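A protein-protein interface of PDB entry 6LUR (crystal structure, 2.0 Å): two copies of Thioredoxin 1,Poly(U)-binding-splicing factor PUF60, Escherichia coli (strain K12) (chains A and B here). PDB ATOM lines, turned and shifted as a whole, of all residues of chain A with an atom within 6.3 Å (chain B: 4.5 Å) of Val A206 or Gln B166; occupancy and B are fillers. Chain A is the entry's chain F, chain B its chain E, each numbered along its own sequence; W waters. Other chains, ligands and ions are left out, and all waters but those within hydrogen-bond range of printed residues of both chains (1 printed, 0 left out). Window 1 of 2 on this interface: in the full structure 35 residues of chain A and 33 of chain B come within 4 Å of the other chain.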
ATOM      1  N   GLU A  95     -30.008   3.575 -17.420  1.00  0.00           N
ATOM      2  CA  GLU A  95     -30.096   2.376 -18.241  1.00  0.00           C
ATOM      3  C   GLU A  95     -31.525   2.238 -18.763  1.00  0.00           C
ATOM      4  O   GLU A  95     -32.467   2.446 -18.010  1.00  0.00           O
ATOM      5  CB  GLU A  95     -29.600   1.162 -17.442  1.00  0.00           C
ATOM      6  CG  GLU A  95     -29.486  -0.104 -18.271  1.00  0.00           C
ATOM      7  CD  GLU A  95     -28.494  -1.113 -17.718  1.00  0.00           C
ATOM      8  OE1 GLU A  95     -28.566  -1.409 -16.522  1.00  0.00           O
ATOM      9  OE2 GLU A  95     -27.628  -1.577 -18.483  1.00  0.00           O
ATOM     10  N   VAL A 128     -20.985 -11.665 -16.120  1.00  0.00           N
ATOM     11  CA  VAL A 128     -20.224 -11.793 -17.357  1.00  0.00           C
ATOM     12  C   VAL A 128     -19.296 -10.586 -17.472  1.00  0.00           C
ATOM     13  O   VAL A 128     -19.716  -9.467 -17.154  1.00  0.00           O
ATOM     14  CB  VAL A 128     -21.115 -11.986 -18.612  1.00  0.00           C
ATOM     15  CG1 VAL A 128     -22.128 -10.864 -18.872  1.00  0.00           C
ATOM     16  CG2 VAL A 128     -20.311 -12.329 -19.870  1.00  0.00           C
ATOM     17  N   LEU A 129     -18.035 -10.849 -17.884  1.00  0.00           N
ATOM     18  CA  LEU A 129     -17.062  -9.800 -18.167  1.00  0.00           C
ATOM     19  C   LEU A 129     -16.901  -9.676 -19.682  1.00  0.00           C
ATOM     20  O   LEU A 129     -16.597 -10.662 -20.346  1.00  0.00           O
ATOM     21  CB  LEU A 129     -15.717 -10.117 -17.489  1.00  0.00           C
ATOM     22  CG  LEU A 129     -15.755 -10.113 -15.961  1.00  0.00           C
ATOM     23  CD1 LEU A 129     -14.492 -10.754 -15.367  1.00  0.00           C
ATOM     24  CD2 LEU A 129     -15.904  -8.685 -15.459  1.00  0.00           C
ATOM     25  N   ARG A 130     -17.207  -8.482 -20.212  1.00  0.00           N
ATOM     26  CA  ARG A 130     -17.147  -8.199 -21.646  1.00  0.00           C
ATOM     27  C   ARG A 130     -16.099  -7.113 -21.878  1.00  0.00           C
ATOM     28  O   ARG A 130     -15.733  -6.361 -20.956  1.00  0.00           O
ATOM     29  CB  ARG A 130     -18.507  -7.745 -22.198  1.00  0.00           C
ATOM     30  CG  ARG A 130     -19.688  -8.647 -21.863  1.00  0.00           C
ATOM     31  CD  ARG A 130     -20.948  -8.056 -22.491  1.00  0.00           C
ATOM     32  NE  ARG A 130     -22.146  -8.617 -21.904  1.00  0.00           N
ATOM     33  CZ  ARG A 130     -22.843  -9.658 -22.385  1.00  0.00           C
ATOM     34  NH1 ARG A 130     -22.490 -10.247 -23.513  1.00  0.00           N
ATOM     35  NH2 ARG A 130     -23.920 -10.102 -21.747  1.00  0.00           N
ATOM     36  N   ASN A 131     -15.526  -7.103 -23.082  1.00  0.00           N
ATOM     37  CA  ASN A 131     -14.538  -6.085 -23.431  1.00  0.00           C
ATOM     38  C   ASN A 131     -13.321  -6.156 -22.491  1.00  0.00           C
ATOM     39  O   ASN A 131     -12.755  -5.139 -22.058  1.00  0.00           O
ATOM     40  CB  ASN A 131     -15.208  -4.701 -23.520  1.00  0.00           C
ATOM     41  CG  ASN A 131     -14.377  -3.641 -24.219  1.00  0.00           C
ATOM     42  OD1 ASN A 131     -13.793  -3.894 -25.267  1.00  0.00           O
ATOM     43  ND2 ASN A 131     -14.308  -2.449 -23.641  1.00  0.00           N
ATOM     44  N   MET A 132     -12.897  -7.372 -22.149  1.00  0.00           N
ATOM     45  CA  MET A 132     -11.775  -7.439 -21.229  1.00  0.00           C
ATOM     46  C   MET A 132     -10.507  -7.980 -21.898  1.00  0.00           C
ATOM     47  O   MET A 132      -9.430  -7.434 -21.691  1.00  0.00           O
ATOM     48  CB  MET A 132     -12.100  -8.237 -19.963  1.00  0.00           C
ATOM     49  CG  MET A 132     -11.363  -7.691 -18.773  1.00  0.00           C
ATOM     50  SD  MET A 132     -11.723  -8.666 -17.306  1.00  0.00           S
ATOM     51  CE  MET A 132     -10.354  -9.820 -17.291  1.00  0.00           C
ATOM     52  N   LEU A 195     -16.193  -4.002 -10.200  1.00  0.00           N
ATOM     53  CA  LEU A 195     -15.449  -4.156 -11.464  1.00  0.00           C
ATOM     54  C   LEU A 195     -16.036  -3.333 -12.610  1.00  0.00           C
ATOM     55  O   LEU A 195     -15.311  -2.961 -13.530  1.00  0.00           O
ATOM     56  CB  LEU A 195     -15.397  -5.633 -11.877  1.00  0.00           C
ATOM     57  CG  LEU A 195     -14.583  -6.560 -10.972  1.00  0.00           C
ATOM     58  CD1 LEU A 195     -14.602  -7.999 -11.497  1.00  0.00           C
ATOM     59  CD2 LEU A 195     -13.144  -6.071 -10.803  1.00  0.00           C
ATOM     60  N   ASN A 196     -17.363  -3.103 -12.607  1.00  0.00           N
ATOM     61  CA  ASN A 196     -18.016  -2.544 -13.780  1.00  0.00           C
ATOM     62  C   ASN A 196     -17.551  -1.107 -13.992  1.00  0.00           C
ATOM     63  O   ASN A 196     -17.653  -0.281 -13.093  1.00  0.00           O
ATOM     64  CB  ASN A 196     -19.538  -2.574 -13.691  1.00  0.00           C
ATOM     65  CG  ASN A 196     -20.186  -2.291 -15.030  1.00  0.00           C
ATOM     66  OD1 ASN A 196     -19.604  -2.592 -16.078  1.00  0.00           O
ATOM     67  ND2 ASN A 196     -21.395  -1.761 -15.003  1.00  0.00           N
ATOM     68  N   GLY A 197     -17.004  -0.823 -15.175  1.00  0.00           N
ATOM     69  CA  GLY A 197     -16.576   0.537 -15.466  1.00  0.00           C
ATOM     70  C   GLY A 197     -15.138   0.830 -15.019  1.00  0.00           C
ATOM     71  O   GLY A 197     -14.647   1.917 -15.270  1.00  0.00           O
ATOM     72  N   ARG A 198     -14.440  -0.133 -14.403  1.00  0.00           N
ATOM     73  CA  ARG A 198     -13.022   0.049 -14.083  1.00  0.00           C
ATOM     74  C   ARG A 198     -12.203  -0.050 -15.371  1.00  0.00           C
ATOM     75  O   ARG A 198     -12.636  -0.684 -16.338  1.00  0.00           O
ATOM     76  CB  ARG A 198     -12.531  -1.052 -13.137  1.00  0.00           C
ATOM     77  CG  ARG A 198     -13.247  -1.108 -11.796  1.00  0.00           C
ATOM     78  CD  ARG A 198     -12.479  -0.286 -10.786  1.00  0.00           C
ATOM     79  NE  ARG A 198     -11.090  -0.730 -10.841  1.00  0.00           N
ATOM     80  CZ  ARG A 198     -10.116  -0.303 -10.044  1.00  0.00           C
ATOM     81  NH1 ARG A 198      -8.889  -0.772 -10.191  1.00  0.00           N
ATOM     82  NH2 ARG A 198     -10.366   0.593  -9.106  1.00  0.00           N
ATOM     83  N   LYS A 204     -12.301   0.066 -20.757  1.00  0.00           N
ATOM     84  CA  LYS A 204     -13.305   0.036 -19.710  1.00  0.00           C
ATOM     85  C   LYS A 204     -13.940  -1.359 -19.652  1.00  0.00           C
ATOM     86  O   LYS A 204     -14.450  -1.864 -20.649  1.00  0.00           O
ATOM     87  CB  LYS A 204     -14.342   1.106 -20.027  1.00  0.00           C
ATOM     88  CG  LYS A 204     -14.812   1.904 -18.833  1.00  0.00           C
ATOM     89  CD  LYS A 204     -15.748   2.977 -19.281  1.00  0.00           C
ATOM     90  CE  LYS A 204     -16.472   3.629 -18.130  1.00  0.00           C
ATOM     91  NZ  LYS A 204     -15.520   4.294 -17.218  1.00  0.00           N
ATOM     92  N   VAL A 205     -13.929  -1.975 -18.468  1.00  0.00           N
ATOM     93  CA  VAL A 205     -14.527  -3.293 -18.335  1.00  0.00           C
ATOM     94  C   VAL A 205     -16.047  -3.139 -18.339  1.00  0.00           C
ATOM     95  O   VAL A 205     -16.579  -2.131 -17.861  1.00  0.00           O
ATOM     96  CB  VAL A 205     -13.954  -4.038 -17.117  1.00  0.00           C
ATOM     97  CG1 VAL A 205     -14.742  -5.300 -16.773  1.00  0.00           C
ATOM     98  CG2 VAL A 205     -12.499  -4.400 -17.405  1.00  0.00           C
ATOM     99  N   VAL A 206     -16.730  -4.110 -18.946  1.00  0.00           N
ATOM    100  CA  VAL A 206     -18.153  -4.284 -18.703  1.00  0.00           C
ATOM    101  C   VAL A 206     -18.361  -5.571 -17.888  1.00  0.00           C
ATOM    102  O   VAL A 206     -18.041  -6.668 -18.333  1.00  0.00           O
ATOM    103  CB  VAL A 206     -18.940  -4.301 -20.022  1.00  0.00           C
ATOM    104  CG1 VAL A 206     -20.403  -4.669 -19.789  1.00  0.00           C
ATOM    105  CG2 VAL A 206     -18.800  -2.971 -20.757  1.00  0.00           C
ATOM    106  N   ALA A 207     -18.830  -5.394 -16.658  1.00  0.00           N
ATOM    107  CA  ALA A 207     -19.183  -6.466 -15.742  1.00  0.00           C
ATOM    108  C   ALA A 207     -20.679  -6.353 -15.502  1.00  0.00           C
ATOM    109  O   ALA A 207     -21.139  -5.294 -15.105  1.00  0.00           O
ATOM    110  CB  ALA A 207     -18.427  -6.297 -14.448  1.00  0.00           C
ATOM    111  N   GLU A 208     -21.443  -7.418 -15.768  1.00  0.00           N
ATOM    112  CA  GLU A 208     -22.879  -7.340 -15.523  1.00  0.00           C
ATOM    113  C   GLU A 208     -23.455  -8.718 -15.189  1.00  0.00           C
ATOM    114  O   GLU A 208     -22.784  -9.744 -15.371  1.00  0.00           O
ATOM    115  CB  GLU A 208     -23.596  -6.587 -16.656  1.00  0.00           C
ATOM    116  CG  GLU A 208     -23.646  -7.322 -17.968  1.00  0.00           C
ATOM    117  CD  GLU A 208     -23.951  -6.489 -19.217  1.00  0.00           C
ATOM    118  OE1 GLU A 208     -23.690  -6.996 -20.320  1.00  0.00           O
ATOM    119  OE2 GLU A 208     -24.454  -5.347 -19.104  1.00  0.00           O
ATOM    120  N   GLU B 164     -26.197   3.644 -25.076  1.00  0.00           N
ATOM    121  CA  GLU B 164     -26.696   2.665 -24.131  1.00  0.00           C
ATOM    122  C   GLU B 164     -25.644   2.480 -23.045  1.00  0.00           C
ATOM    123  O   GLU B 164     -24.480   2.227 -23.341  1.00  0.00           O
ATOM    124  CB  GLU B 164     -26.950   1.344 -24.861  1.00  0.00           C
ATOM    125  CG  GLU B 164     -27.470   0.250 -23.950  1.00  0.00           C
ATOM    126  CD  GLU B 164     -27.493  -1.098 -24.638  1.00  0.00           C
ATOM    127  OE1 GLU B 164     -26.428  -1.768 -24.664  1.00  0.00           O
ATOM    128  OE2 GLU B 164     -28.545  -1.436 -25.222  1.00  0.00           O
ATOM    129  N   LYS B 165     -26.078   2.616 -21.789  1.00  0.00           N
ATOM    130  CA  LYS B 165     -25.179   2.485 -20.656  1.00  0.00           C
ATOM    131  C   LYS B 165     -25.157   1.006 -20.299  1.00  0.00           C
ATOM    132  O   LYS B 165     -26.202   0.374 -20.338  1.00  0.00           O
ATOM    133  CB  LYS B 165     -25.639   3.396 -19.519  1.00  0.00           C
ATOM    134  CG  LYS B 165     -24.790   3.332 -18.255  1.00  0.00           C
ATOM    135  CD  LYS B 165     -25.393   4.181 -17.151  1.00  0.00           C
ATOM    136  CE  LYS B 165     -24.885   3.808 -15.775  1.00  0.00           C
ATOM    137  NZ  LYS B 165     -25.662   4.487 -14.732  1.00  0.00           N
ATOM    138  N   GLN B 166     -23.965   0.475 -20.001  1.00  0.00           N
ATOM    139  CA  GLN B 166     -23.752  -0.942 -19.772  1.00  0.00           C
ATOM    140  C   GLN B 166     -23.873  -1.248 -18.281  1.00  0.00           C
ATOM    141  O   GLN B 166     -22.878  -1.494 -17.607  1.00  0.00           O
ATOM    142  CB  GLN B 166     -22.386  -1.335 -20.324  1.00  0.00           C
ATOM    143  CG  GLN B 166     -22.246  -1.056 -21.814  1.00  0.00           C
ATOM    144  CD  GLN B 166     -23.362  -1.750 -22.546  1.00  0.00           C
ATOM    145  OE1 GLN B 166     -23.384  -2.977 -22.630  1.00  0.00           O
ATOM    146  NE2 GLN B 166     -24.310  -0.975 -23.050  1.00  0.00           N
ATOM    147  N   GLY B 167     -25.104  -1.242 -17.774  1.00  0.00           N
ATOM    148  CA  GLY B 167     -25.327  -1.498 -16.358  1.00  0.00           C
ATOM    149  C   GLY B 167     -25.673  -0.230 -15.584  1.00  0.00           C
ATOM    150  O   GLY B 167     -25.522   0.883 -16.079  1.00  0.00           O
ATOM    151  N   ALA B 172     -20.400   2.975 -15.394  1.00  0.00           N
ATOM    152  CA  ALA B 172     -20.660   2.050 -16.479  1.00  0.00           C
ATOM    153  C   ALA B 172     -20.300   2.715 -17.800  1.00  0.00           C
ATOM    154  O   ALA B 172     -20.510   3.913 -18.002  1.00  0.00           O
ATOM    155  CB  ALA B 172     -22.101   1.594 -16.467  1.00  0.00           C
ATOM    156  N   GLU B 173     -19.757   1.910 -18.708  1.00  0.00           N
ATOM    157  CA  GLU B 173     -19.444   2.383 -20.048  1.00  0.00           C
ATOM    158  C   GLU B 173     -20.713   2.716 -20.848  1.00  0.00           C
ATOM    159  O   GLU B 173     -21.738   2.056 -20.724  1.00  0.00           O
ATOM    160  CB  GLU B 173     -18.688   1.266 -20.745  1.00  0.00           C
ATOM    161  CG  GLU B 173     -18.282   1.611 -22.165  1.00  0.00           C
ATOM    162  CD  GLU B 173     -17.664   0.402 -22.837  1.00  0.00           C
ATOM    163  OE1 GLU B 173     -18.314  -0.654 -22.862  1.00  0.00           O
ATOM    164  OE2 GLU B 173     -16.523   0.508 -23.292  1.00  0.00           O
ATOM    165  N   ILE B 175     -21.953   2.851 -24.683  1.00  0.00           N
ATOM    166  CA  ILE B 175     -21.566   2.430 -26.020  1.00  0.00           C
ATOM    167  C   ILE B 175     -22.569   2.985 -27.035  1.00  0.00           C
ATOM    168  O   ILE B 175     -23.661   3.415 -26.679  1.00  0.00           O
ATOM    169  CB  ILE B 175     -21.384   0.899 -26.136  1.00  0.00           C
ATOM    170  CG1 ILE B 175     -22.602   0.122 -25.624  1.00  0.00           C
ATOM    171  CG2 ILE B 175     -20.097   0.430 -25.456  1.00  0.00           C
ATOM    172  CD1 ILE B 175     -23.506  -0.394 -26.701  1.00  0.00           C
HETATM  173  O   HOH W   1     -19.100  -0.844 -18.042  1.00  0.00           O
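The side-chain amide nitrogen of Asn A196 lies within hydrogen-bond range of the backbone carbonyl oxygen of Gln B166 (3.0 Å).
The backbone NH (N) of Gly B167 is in hydrogen-bond range of the side-chain carboxylate (OE2) of Glu A95 (2.6 Å).
The backbone carbonyl oxygen (O) of Lys B165 lies close to the side-chain carboxylate (OE2) of Glu A95 (3.0 Å).
OE1 of Glu B164 sits at hydrogen-bond distance from NE2 of Gln B166 (2.8 Å).
N of Gln B166 sits at hydrogen-bond distance from O of Glu B173, at 2.8 Å.
O of Val A206 lies within hydrogen-bond range of N of Arg A130, 2.7 Å away.
The side-chain amide nitrogen (ND2) of Asn A131 sits at hydrogen-bond distance from the backbone carbonyl oxygen (O) of Lys A204 (3.1 Å).
OD1 of Asn A196 is in hydrogen-bond range of N of Ala A207 (3.0 Å).
The backbone carbonyl oxygen (O) of Gly A197 sits at hydrogen-bond distance from the side-chain amino group (NZ) of Lys A204, at 3.2 Å.
Among the printed residues, merely in contact across the chains: Val A206 with Glu B173 (3.2 Å), Lys A204 with Glu B173 (3.7 Å), Asn A131 with Glu B173 (3.7 Å), Asn A196 with Ala B172 (3.7 Å), Glu A95 with Gln B166 (3.8 Å), Val A206 with Gln B166 (3.9 Å) and Lys A204 with Ala B172 (3.9 Å).
Of the printed residues of chain B, Glu A95 touches Lys B165 (3.0 Å), Gln B166 (3.8 Å) and Gly B167 (2.6 Å).
Of the printed residues of chain B, Asn A196 touches Gln B166 (3.0 Å) and Ala B172 (3.7 Å).
Of the printed residues of chain B, Lys A204 touches Ala B172 (3.9 Å) and Glu B173 (3.7 Å).
Val A206 touches two residues of chain B.
Gln B166 touches just these residues of chain A: Glu A95, Asn A196 and Val A206.
Printed residues of chain A within 4 Å of Gly B167: Glu A95.
Of the printed residues of chain A, Glu B173 touches Asn A131 (3.7 Å), Lys A204 (3.7 Å) and Val A206 (3.2 Å).
The nearest printed residue of chain B that does not touch Val A206 is Ile B175 (5.9 Å).
The nearest printed residue of chain B that does not touch Asn A131 is Ile B175 (6.7 Å).
Of the 7 printed residues of chain B, 5 touch a printed residue of chain A.
Printed residues of chain B that touch a printed residue of chain A: Lys B165, Gln B166, Gly B167, Ala B172 and Glu B173.
Hydrophobic or aromatic side chains of chain A that line the printed part of chain B: Val A206.
Among the printed residues, no Asp or Glu carboxylate lies within 4 Å of a Lys or Arg side-chain nitrogen of the other chain.
No position is printed for both chains.
Water W1 lies within hydrogen-bond range of OD1 of Asn A196, O of Val A205 and N of Glu B173.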
